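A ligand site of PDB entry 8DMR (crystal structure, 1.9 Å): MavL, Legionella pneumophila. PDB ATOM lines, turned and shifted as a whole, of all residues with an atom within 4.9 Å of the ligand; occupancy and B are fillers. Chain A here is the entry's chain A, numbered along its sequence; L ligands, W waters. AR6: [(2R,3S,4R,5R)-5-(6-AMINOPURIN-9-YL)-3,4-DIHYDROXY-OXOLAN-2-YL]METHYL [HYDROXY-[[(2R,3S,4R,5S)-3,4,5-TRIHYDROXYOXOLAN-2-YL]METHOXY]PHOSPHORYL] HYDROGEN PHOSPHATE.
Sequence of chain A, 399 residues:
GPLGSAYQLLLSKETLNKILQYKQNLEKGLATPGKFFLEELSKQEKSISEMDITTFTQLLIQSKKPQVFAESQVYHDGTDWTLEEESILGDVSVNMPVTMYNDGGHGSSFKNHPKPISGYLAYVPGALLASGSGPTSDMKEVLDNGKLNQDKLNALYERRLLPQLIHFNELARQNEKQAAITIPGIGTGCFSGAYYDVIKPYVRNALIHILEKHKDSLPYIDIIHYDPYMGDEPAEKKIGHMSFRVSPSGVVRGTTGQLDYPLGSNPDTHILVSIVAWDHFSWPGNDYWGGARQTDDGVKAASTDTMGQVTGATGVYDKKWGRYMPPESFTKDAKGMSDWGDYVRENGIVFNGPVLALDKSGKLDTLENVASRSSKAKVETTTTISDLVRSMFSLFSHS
OD2 of Asp 279 is in hydrogen-bond range of ND2 of Asn 286 (3.4 Å). OD2 of Asp 279 is in hydrogen-bond range of N of Ala 70 (2.9 Å). The backbone carbonyl oxygen (O) of Gly 189 is in hydrogen-bond range of the side-chain hydroxyl (OG) of Ser 192 (2.6 Å). OD1 of Asp 287 sits at hydrogen-bond distance from OG1 of Thr 295. The backbone NH (N) of Val 68 lies within hydrogen-bond range of the side-chain amide oxygen (OD1) of Asn 286, at 2.8 Å. The side-chain hydroxyl (OG1) of Thr 188 lies within hydrogen-bond range of the backbone carbonyl oxygen (O) of Gly 185 (2.7 Å). The side-chain hydroxyl (OG1) of Thr 188 is in hydrogen-bond range of the side-chain amino group (NZ) of Lys 200 (3.0 Å). O of Pro 228 lies within hydrogen-bond range of NZ of Lys 200, at 3.1 Å.
The side-chain carboxylate of Asp 279 is in hydrogen-bond range of an oxygen (O3D) of the ligand, 2.5 Å away. OD2 of Asp 297 lies within hydrogen-bond range of O2D of the ligand (2.6 Å). The backbone NH of Gly 189 lies within hydrogen-bond range of an oxygen (O2B) of the ligand. The backbone NH of Cys 190 is in hydrogen-bond range of an oxygen (O1A) of the ligand (2.8 Å). An oxygen (O1A) of the ligand is in hydrogen-bond range of the side-chain sulfur (SG) of Cys 190, at 3.5 Å. OD1 of Asp 287 sits at hydrogen-bond distance from O1D of the ligand (2.8 Å). An oxygen (O1B) of the ligand lies within hydrogen-bond range of the backbone NH of Gly 187 (2.9 Å). An oxygen (O2D) of the ligand is in hydrogen-bond range of the side-chain amide nitrogen (ND2) of Asn 286 (2.9 Å). An oxygen (O2B) of the ligand sits at hydrogen-bond distance from the backbone NH (N) of Thr 188 (3.4 Å). The side-chain hydroxyl of Thr 188 sits at hydrogen-bond distance from an oxygen (O3') of the ligand (2.9 Å). The backbone NH of Asp 296 sits at hydrogen-bond distance from an oxygen (O2A) of the ligand, 3.1 Å away. The backbone NH (N) of Phe 191 lies within hydrogen-bond range of an oxygen (O2B) of the ligand, at 3.1 Å. The backbone carbonyl oxygen of Pro 228 lies within hydrogen-bond range of an oxygen (O3') of the ligand. The backbone carbonyl oxygen (O) of Gly 185 is in hydrogen-bond range of an oxygen (O3') of the ligand (3.3 Å). O3' of the ligand lies within hydrogen-bond range of NZ of Lys 200, at 3.4 Å.
CG of His 106 touches N1 of the ligand (3.3 Å). Tyr 229 touches the ligand (CD1 to C2, 3.4 Å). Ala 277 touches the ligand. Trp 278 touches the ligand. Thr 295 touches the ligand (OG1 to C1D, 3.3 Å).
Water W6 lies within hydrogen-bond range of an oxygen (O2') of the ligand (2.6 Å) and the backbone carbonyl oxygen (O) of Thr 188 (2.7 Å). Water W9 bridges an oxygen (O1A) of the ligand and the side-chain sulfur of Cys 190. Water W1 lies within hydrogen-bond range of O2A of the ligand (2.8 Å) and N of Asp 296 (3.4 Å). Water W11 lies within hydrogen-bond range of the backbone carbonyl oxygen (O) of Ala 277 (2.7 Å), an oxygen (O2A) of the ligand (2.8 Å), the backbone NH (N) of Asp 297 (2.9 Å) and the backbone NH (N) of Asp 296 (3.4 Å). Water W4 lies within hydrogen-bond range of OD2 of Asp 287 (2.8 Å) and O1D of the ligand (3.0 Å). Water W7 lies within hydrogen-bond range of the backbone NH (N) of Gly 185 and an oxygen (O3') of the ligand.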
ATOM      1  N   VAL A  68      -2.942   2.472  11.456  1.00  0.00           N
ATOM      2  CA  VAL A  68      -2.044   1.491  10.867  1.00  0.00           C
ATOM      3  C   VAL A  68      -2.766   0.800   9.729  1.00  0.00           C
ATOM      4  O   VAL A  68      -3.914   0.368   9.883  1.00  0.00           O
ATOM      5  CB  VAL A  68      -1.507   0.512  11.932  1.00  0.00           C
ATOM      6  CG1 VAL A  68      -2.584  -0.142  12.678  1.00  0.00           C
ATOM      7  CG2 VAL A  68      -0.687  -0.605  11.238  1.00  0.00           C
ATOM      8  N   PHE A  69      -2.124   0.764   8.566  1.00  0.00           N
ATOM      9  CA  PHE A  69      -2.699   0.170   7.371  1.00  0.00           C
ATOM     10  C   PHE A  69      -2.260  -1.280   7.245  1.00  0.00           C
ATOM     11  O   PHE A  69      -1.115  -1.558   6.901  1.00  0.00           O
ATOM     12  CB  PHE A  69      -2.270   0.962   6.147  1.00  0.00           C
ATOM     13  CG  PHE A  69      -2.677   2.407   6.191  1.00  0.00           C
ATOM     14  CD1 PHE A  69      -3.921   2.738   6.683  1.00  0.00           C
ATOM     15  CD2 PHE A  69      -1.838   3.397   5.720  1.00  0.00           C
ATOM     16  CE1 PHE A  69      -4.326   4.061   6.735  1.00  0.00           C
ATOM     17  CE2 PHE A  69      -2.224   4.723   5.764  1.00  0.00           C
ATOM     18  CZ  PHE A  69      -3.491   5.058   6.257  1.00  0.00           C
ATOM     19  N   ALA A  70      -3.188  -2.197   7.512  1.00  0.00           N
ATOM     20  CA  ALA A  70      -2.890  -3.618   7.378  1.00  0.00           C
ATOM     21  C   ALA A  70      -2.413  -3.973   5.985  1.00  0.00           C
ATOM     22  O   ALA A  70      -1.588  -4.881   5.823  1.00  0.00           O
ATOM     23  CB  ALA A  70      -4.142  -4.442   7.726  1.00  0.00           C
ATOM     24  N   HIS A 106     -17.719  10.249  -0.042  1.00  0.00           N
ATOM     25  CA  HIS A 106     -16.275  10.438  -0.015  1.00  0.00           C
ATOM     26  C   HIS A 106     -15.906  11.759  -0.677  1.00  0.00           C
ATOM     27  O   HIS A 106     -16.685  12.346  -1.438  1.00  0.00           O
ATOM     28  CB  HIS A 106     -15.577   9.289  -0.724  1.00  0.00           C
ATOM     29  CG  HIS A 106     -15.722   7.977  -0.024  1.00  0.00           C
ATOM     30  ND1 HIS A 106     -14.742   7.005  -0.056  1.00  0.00           N
ATOM     31  CD2 HIS A 106     -16.716   7.492   0.751  1.00  0.00           C
ATOM     32  CE1 HIS A 106     -15.135   5.964   0.664  1.00  0.00           C
ATOM     33  NE2 HIS A 106     -16.332   6.240   1.168  1.00  0.00           N
ATOM     34  N   PRO A 184     -21.096  -1.506   3.230  1.00  0.00           N
ATOM     35  CA  PRO A 184     -20.261  -1.181   2.072  1.00  0.00           C
ATOM     36  C   PRO A 184     -19.662  -2.437   1.471  1.00  0.00           C
ATOM     37  O   PRO A 184     -19.886  -3.559   1.963  1.00  0.00           O
ATOM     38  CB  PRO A 184     -19.167  -0.272   2.676  1.00  0.00           C
ATOM     39  CG  PRO A 184     -18.917  -0.966   4.058  1.00  0.00           C
ATOM     40  CD  PRO A 184     -20.327  -1.485   4.491  1.00  0.00           C
ATOM     41  N   GLY A 185     -18.862  -2.271   0.425  1.00  0.00           N
ATOM     42  CA  GLY A 185     -18.165  -3.412  -0.131  1.00  0.00           C
ATOM     43  C   GLY A 185     -16.936  -3.794   0.681  1.00  0.00           C
ATOM     44  O   GLY A 185     -15.785  -3.526   0.263  1.00  0.00           O
ATOM     45  N   ILE A 186     -17.173  -4.407   1.834  1.00  0.00           N
ATOM     46  CA  ILE A 186     -16.093  -4.725   2.760  1.00  0.00           C
ATOM     47  C   ILE A 186     -15.104  -5.677   2.114  1.00  0.00           C
ATOM     48  O   ILE A 186     -15.463  -6.689   1.486  1.00  0.00           O
ATOM     49  CB  ILE A 186     -16.703  -5.273   4.072  1.00  0.00           C
ATOM     50  CG1 ILE A 186     -15.661  -5.637   5.096  1.00  0.00           C
ATOM     51  CG2 ILE A 186     -17.590  -6.456   3.788  1.00  0.00           C
ATOM     52  CD1 ILE A 186     -16.275  -5.847   6.534  1.00  0.00           C
ATOM     53  N   GLY A 187     -13.822  -5.347   2.258  1.00  0.00           N
ATOM     54  CA  GLY A 187     -12.776  -6.168   1.695  1.00  0.00           C
ATOM     55  C   GLY A 187     -12.495  -5.974   0.218  1.00  0.00           C
ATOM     56  O   GLY A 187     -11.584  -6.632  -0.312  1.00  0.00           O
ATOM     57  N   THR A 188     -13.218  -5.113  -0.479  1.00  0.00           N
ATOM     58  CA  THR A 188     -13.122  -5.062  -1.931  1.00  0.00           C
ATOM     59  C   THR A 188     -12.295  -3.881  -2.430  1.00  0.00           C
ATOM     60  O   THR A 188     -12.233  -3.645  -3.655  1.00  0.00           O
ATOM     61  CB  THR A 188     -14.511  -5.020  -2.557  1.00  0.00           C
ATOM     62  OG1 THR A 188     -15.118  -3.754  -2.308  1.00  0.00           O
ATOM     63  CG2 THR A 188     -15.401  -6.133  -2.049  1.00  0.00           C
ATOM     64  N   GLY A 189     -11.679  -3.123  -1.535  1.00  0.00           N
ATOM     65  CA  GLY A 189     -10.798  -2.048  -1.926  1.00  0.00           C
ATOM     66  C   GLY A 189      -9.366  -2.293  -1.461  1.00  0.00           C
ATOM     67  O   GLY A 189      -8.654  -3.101  -2.051  1.00  0.00           O
ATOM     68  N   CYS A 190      -8.947  -1.578  -0.402  1.00  0.00           N
ATOM     69  CA  CYS A 190      -7.571  -1.667   0.073  1.00  0.00           C
ATOM     70  C   CYS A 190      -7.191  -3.079   0.496  1.00  0.00           C
ATOM     71  O   CYS A 190      -6.008  -3.435   0.439  1.00  0.00           O
ATOM     72  CB  CYS A 190      -7.355  -0.719   1.267  1.00  0.00           C
ATOM     73  SG  CYS A 190      -7.477   1.009   0.959  1.00  0.00           S
ATOM     74  N   PHE A 191      -8.160  -3.886   0.942  1.00  0.00           N
ATOM     75  CA  PHE A 191      -7.884  -5.228   1.430  1.00  0.00           C
ATOM     76  C   PHE A 191      -7.930  -6.283   0.334  1.00  0.00           C
ATOM     77  O   PHE A 191      -7.705  -7.465   0.614  1.00  0.00           O
ATOM     78  CB  PHE A 191      -8.877  -5.608   2.560  1.00  0.00           C
ATOM     79  CG  PHE A 191      -8.438  -5.183   3.933  1.00  0.00           C
ATOM     80  CD1 PHE A 191      -7.424  -4.269   4.123  1.00  0.00           C
ATOM     81  CD2 PHE A 191      -9.044  -5.718   5.079  1.00  0.00           C
ATOM     82  CE1 PHE A 191      -6.996  -3.889   5.375  1.00  0.00           C
ATOM     83  CE2 PHE A 191      -8.623  -5.324   6.348  1.00  0.00           C
ATOM     84  CZ  PHE A 191      -7.625  -4.414   6.499  1.00  0.00           C
ATOM     85  N   SER A 192      -8.207  -5.898  -0.927  1.00  0.00           N
ATOM     86  CA  SER A 192      -8.454  -6.889  -1.980  1.00  0.00           C
ATOM     87  C   SER A 192      -7.177  -7.396  -2.647  1.00  0.00           C
ATOM     88  O   SER A 192      -7.158  -8.523  -3.160  1.00  0.00           O
ATOM     89  CB  SER A 192      -9.363  -6.285  -3.059  1.00  0.00           C
ATOM     90  OG  SER A 192      -8.740  -5.180  -3.680  1.00  0.00           O
ATOM     91  N   LYS A 200     -15.657  -8.887  -5.734  1.00  0.00           N
ATOM     92  CA  LYS A 200     -16.938  -8.267  -5.388  1.00  0.00           C
ATOM     93  C   LYS A 200     -18.083  -9.259  -5.323  1.00  0.00           C
ATOM     94  O   LYS A 200     -18.870  -9.196  -4.358  1.00  0.00           O
ATOM     95  CB  LYS A 200     -17.249  -7.139  -6.379  1.00  0.00           C
ATOM     96  CG  LYS A 200     -16.323  -5.951  -6.157  1.00  0.00           C
ATOM     97  CD  LYS A 200     -16.861  -4.633  -6.674  1.00  0.00           C
ATOM     98  CE  LYS A 200     -15.925  -3.450  -6.303  1.00  0.00           C
ATOM     99  NZ  LYS A 200     -16.339  -2.912  -4.944  1.00  0.00           N
ATOM    100  N   PRO A 228     -21.845  -1.665  -2.795  1.00  0.00           N
ATOM    101  CA  PRO A 228     -20.446  -1.931  -3.159  1.00  0.00           C
ATOM    102  C   PRO A 228     -19.793  -0.807  -3.957  1.00  0.00           C
ATOM    103  O   PRO A 228     -18.658  -0.962  -4.405  1.00  0.00           O
ATOM    104  CB  PRO A 228     -20.559  -3.195  -4.008  1.00  0.00           C
ATOM    105  CG  PRO A 228     -21.888  -3.016  -4.722  1.00  0.00           C
ATOM    106  CD  PRO A 228     -22.788  -2.323  -3.717  1.00  0.00           C
ATOM    107  N   TYR A 229     -20.516   0.292  -4.123  1.00  0.00           N
ATOM    108  CA  TYR A 229     -20.122   1.514  -4.844  1.00  0.00           C
ATOM    109  C   TYR A 229     -20.136   1.302  -6.348  1.00  0.00           C
ATOM    110  O   TYR A 229     -20.896   1.953  -7.063  1.00  0.00           O
ATOM    111  CB  TYR A 229     -18.745   2.027  -4.433  1.00  0.00           C
ATOM    112  CG  TYR A 229     -18.555   3.462  -4.876  1.00  0.00           C
ATOM    113  CD1 TYR A 229     -19.547   4.415  -4.621  1.00  0.00           C
ATOM    114  CD2 TYR A 229     -17.449   3.856  -5.607  1.00  0.00           C
ATOM    115  CE1 TYR A 229     -19.412   5.725  -5.040  1.00  0.00           C
ATOM    116  CE2 TYR A 229     -17.314   5.180  -6.044  1.00  0.00           C
ATOM    117  CZ  TYR A 229     -18.304   6.099  -5.747  1.00  0.00           C
ATOM    118  OH  TYR A 229     -18.213   7.416  -6.135  1.00  0.00           O
ATOM    119  N   ALA A 277     -15.902  -0.900   7.184  1.00  0.00           N
ATOM    120  CA  ALA A 277     -14.851  -1.821   6.748  1.00  0.00           C
ATOM    121  C   ALA A 277     -13.587  -1.413   7.496  1.00  0.00           C
ATOM    122  O   ALA A 277     -12.895  -0.461   7.104  1.00  0.00           O
ATOM    123  CB  ALA A 277     -14.631  -1.735   5.240  1.00  0.00           C
ATOM    124  N   TRP A 278     -13.302  -2.145   8.560  1.00  0.00           N
ATOM    125  CA  TRP A 278     -12.308  -1.776   9.561  1.00  0.00           C
ATOM    126  C   TRP A 278     -10.952  -2.409   9.232  1.00  0.00           C
ATOM    127  O   TRP A 278     -10.660  -2.780   8.094  1.00  0.00           O
ATOM    128  CB  TRP A 278     -12.817  -2.229  10.942  1.00  0.00           C
ATOM    129  CG  TRP A 278     -12.146  -1.638  12.153  1.00  0.00           C
ATOM    130  CD1 TRP A 278     -11.289  -0.567  12.194  1.00  0.00           C
ATOM    131  CD2 TRP A 278     -12.207  -2.165  13.469  1.00  0.00           C
ATOM    132  NE1 TRP A 278     -10.832  -0.388  13.484  1.00  0.00           N
ATOM    133  CE2 TRP A 278     -11.405  -1.346  14.281  1.00  0.00           C
ATOM    134  CE3 TRP A 278     -12.897  -3.229  14.051  1.00  0.00           C
ATOM    135  CZ2 TRP A 278     -11.285  -1.553  15.659  1.00  0.00           C
ATOM    136  CZ3 TRP A 278     -12.753  -3.447  15.405  1.00  0.00           C
ATOM    137  CH2 TRP A 278     -11.964  -2.617  16.190  1.00  0.00           C
ATOM    138  N   ASP A 279     -10.072  -2.495  10.247  1.00  0.00           N
ATOM    139  CA  ASP A 279      -8.688  -2.939  10.112  1.00  0.00           C
ATOM    140  C   ASP A 279      -8.299  -3.735  11.366  1.00  0.00           C
ATOM    141  O   ASP A 279      -8.447  -3.229  12.482  1.00  0.00           O
ATOM    142  CB  ASP A 279      -7.741  -1.746   9.947  1.00  0.00           C
ATOM    143  CG  ASP A 279      -6.358  -2.134   9.498  1.00  0.00           C
ATOM    144  OD1 ASP A 279      -5.662  -2.792  10.317  1.00  0.00           O
ATOM    145  OD2 ASP A 279      -5.907  -1.729   8.401  1.00  0.00           O
ATOM    146  N   SER A 282      -5.976  -1.528  13.715  1.00  0.00           N
ATOM    147  CA  SER A 282      -6.099  -0.108  14.024  1.00  0.00           C
ATOM    148  C   SER A 282      -7.302   0.144  14.918  1.00  0.00           C
ATOM    149  O   SER A 282      -8.200  -0.680  15.060  1.00  0.00           O
ATOM    150  CB  SER A 282      -6.267   0.782  12.783  1.00  0.00           C
ATOM    151  OG  SER A 282      -7.580   0.631  12.306  1.00  0.00           O
ATOM    152  N   ASN A 286      -9.227   4.482  11.661  1.00  0.00           N
ATOM    153  CA  ASN A 286      -7.870   4.364  11.103  1.00  0.00           C
ATOM    154  C   ASN A 286      -7.333   5.631  10.425  1.00  0.00           C
ATOM    155  O   ASN A 286      -6.738   6.467  11.096  1.00  0.00           O
ATOM    156  CB  ASN A 286      -7.864   3.195  10.108  1.00  0.00           C
ATOM    157  CG  ASN A 286      -6.447   2.608   9.887  1.00  0.00           C
ATOM    158  OD1 ASN A 286      -5.462   3.143  10.370  1.00  0.00           O
ATOM    159  ND2 ASN A 286      -6.380   1.521   9.118  1.00  0.00           N
ATOM    160  N   ASP A 287      -7.493   5.753   9.098  1.00  0.00           N
ATOM    161  CA  ASP A 287      -6.894   6.862   8.347  1.00  0.00           C
ATOM    162  C   ASP A 287      -7.148   8.218   8.995  1.00  0.00           C
ATOM    163  O   ASP A 287      -6.290   9.118   8.943  1.00  0.00           O
ATOM    164  CB  ASP A 287      -7.479   6.912   6.926  1.00  0.00           C
ATOM    165  CG  ASP A 287      -7.410   5.589   6.195  1.00  0.00           C
ATOM    166  OD1 ASP A 287      -8.020   4.616   6.694  1.00  0.00           O
ATOM    167  OD2 ASP A 287      -6.822   5.566   5.091  1.00  0.00           O
ATOM    168  N   THR A 295     -11.138   6.394   2.682  1.00  0.00           N
ATOM    169  CA  THR A 295     -11.644   5.025   2.799  1.00  0.00           C
ATOM    170  C   THR A 295     -12.929   4.990   3.618  1.00  0.00           C
ATOM    171  O   THR A 295     -13.273   5.955   4.307  1.00  0.00           O
ATOM    172  CB  THR A 295     -10.599   4.071   3.415  1.00  0.00           C
ATOM    173  OG1 THR A 295     -10.556   4.183   4.844  1.00  0.00           O
ATOM    174  CG2 THR A 295      -9.214   4.299   2.754  1.00  0.00           C
ATOM    175  N   ASP A 296     -13.660   3.869   3.516  1.00  0.00           N
ATOM    176  CA  ASP A 296     -14.915   3.743   4.265  1.00  0.00           C
ATOM    177  C   ASP A 296     -14.684   3.995   5.753  1.00  0.00           C
ATOM    178  O   ASP A 296     -15.436   4.727   6.400  1.00  0.00           O
ATOM    179  CB  ASP A 296     -15.516   2.356   4.000  1.00  0.00           C
ATOM    180  CG  ASP A 296     -16.829   2.144   4.707  1.00  0.00           C
ATOM    181  OD1 ASP A 296     -17.854   2.663   4.248  1.00  0.00           O
ATOM    182  OD2 ASP A 296     -16.851   1.398   5.691  1.00  0.00           O
ATOM    183  N   ASP A 297     -13.592   3.450   6.281  1.00  0.00           N
ATOM    184  CA  ASP A 297     -13.278   3.571   7.706  1.00  0.00           C
ATOM    185  C   ASP A 297     -13.023   5.026   8.087  1.00  0.00           C
ATOM    186  O   ASP A 297     -13.606   5.539   9.041  1.00  0.00           O
ATOM    187  CB  ASP A 297     -12.056   2.690   7.964  1.00  0.00           C
ATOM    188  CG  ASP A 297     -11.866   2.313   9.412  1.00  0.00           C
ATOM    189  OD1 ASP A 297     -12.634   2.750  10.289  1.00  0.00           O
ATOM    190  OD2 ASP A 297     -10.908   1.524   9.658  1.00  0.00           O
HETATM  191  N1  AR6 L   1     -17.171   6.500  -2.585  1.00  0.00           N
HETATM  192  C2  AR6 L   1     -17.741   5.454  -1.970  1.00  0.00           C
HETATM  193  N3  AR6 L   1     -17.276   4.218  -1.820  1.00  0.00           N
HETATM  194  C4  AR6 L   1     -16.079   4.090  -2.396  1.00  0.00           C
HETATM  195  C5  AR6 L   1     -15.369   5.058  -3.073  1.00  0.00           C
HETATM  196  C6  AR6 L   1     -15.957   6.339  -3.157  1.00  0.00           C
HETATM  197  N6  AR6 L   1     -15.392   7.377  -3.761  1.00  0.00           N
HETATM  198  N7  AR6 L   1     -14.162   4.534  -3.526  1.00  0.00           N
HETATM  199  C8  AR6 L   1     -14.173   3.276  -3.133  1.00  0.00           C
HETATM  200  N9  AR6 L   1     -15.309   2.962  -2.415  1.00  0.00           N
HETATM  201  PA  AR6 L   1     -12.129   0.135   1.448  1.00  0.00           P
HETATM  202  PB  AR6 L   1     -11.367  -2.523   2.542  1.00  0.00           P
HETATM  203  C1' AR6 L   1     -15.749   1.699  -1.893  1.00  0.00           C
HETATM  204  O1A AR6 L   1     -10.824   0.127   0.712  1.00  0.00           O
HETATM  205  O1B AR6 L   1     -12.183  -3.331   3.525  1.00  0.00           O
HETATM  206  C1D AR6 L   1      -9.139   1.290   5.495  1.00  0.00           C
HETATM  207  O1D AR6 L   1      -7.942   1.993   5.639  1.00  0.00           O
HETATM  208  C2' AR6 L   1     -14.960   0.558  -2.517  1.00  0.00           C
HETATM  209  O2' AR6 L   1     -15.187   0.112  -3.842  1.00  0.00           O
HETATM  210  O2A AR6 L   1     -12.495   1.345   2.237  1.00  0.00           O
HETATM  211  O2B AR6 L   1     -11.118  -3.080   1.176  1.00  0.00           O
HETATM  212  C2D AR6 L   1      -9.383   0.428   6.737  1.00  0.00           C
HETATM  213  O2D AR6 L   1      -8.992   1.016   7.962  1.00  0.00           O
HETATM  214  C3' AR6 L   1     -15.309  -0.577  -1.526  1.00  0.00           C
HETATM  215  O3' AR6 L   1     -16.496  -1.214  -1.982  1.00  0.00           O
HETATM  216  O3A AR6 L   1     -12.124  -1.125   2.443  1.00  0.00           O
HETATM  217  C3D AR6 L   1      -8.474  -0.760   6.425  1.00  0.00           C
HETATM  218  O3D AR6 L   1      -7.108  -0.432   6.634  1.00  0.00           O
HETATM  219  C4' AR6 L   1     -15.582   0.146  -0.203  1.00  0.00           C
HETATM  220  O4' AR6 L   1     -15.489   1.562  -0.520  1.00  0.00           O
HETATM  221  C4D AR6 L   1      -8.757  -0.966   4.937  1.00  0.00           C
HETATM  222  O4D AR6 L   1      -9.046   0.357   4.411  1.00  0.00           O
HETATM  223  C5' AR6 L   1     -14.637  -0.158   0.929  1.00  0.00           C
HETATM  224  O5' AR6 L   1     -13.302  -0.220   0.419  1.00  0.00           O
HETATM  225  C5D AR6 L   1      -9.947  -1.841   4.636  1.00  0.00           C
HETATM  226  O5D AR6 L   1      -9.990  -2.096   3.226  1.00  0.00           O
HETATM  227  O   HOH W   1     -13.210   3.221   0.220  1.00  0.00           O
HETATM  228  O   HOH W   2     -16.610  10.109  -4.218  1.00  0.00           O
HETATM  229  O   HOH W   3     -18.723   2.996   0.067  1.00  0.00           O
HETATM  230  O   HOH W   4      -6.024   3.240   3.704  1.00  0.00           O
HETATM  231  O   HOH W   5     -18.795   8.658  -2.164  1.00  0.00           O
HETATM  232  O   HOH W   6     -13.048  -1.269  -4.575  1.00  0.00           O
HETATM  233  O   HOH W   7     -18.801   0.374  -0.809  1.00  0.00           O
HETATM  234  O   HOH W   8      -4.876  -1.075   4.928  1.00  0.00           O
HETATM  235  O   HOH W   9     -10.209   1.655  -1.453  1.00  0.00           O
HETATM  236  O   HOH W  10     -12.304  -3.998   6.108  1.00  0.00           O
HETATM  237  O   HOH W  11     -12.302   1.135   5.070  1.00  0.00           O
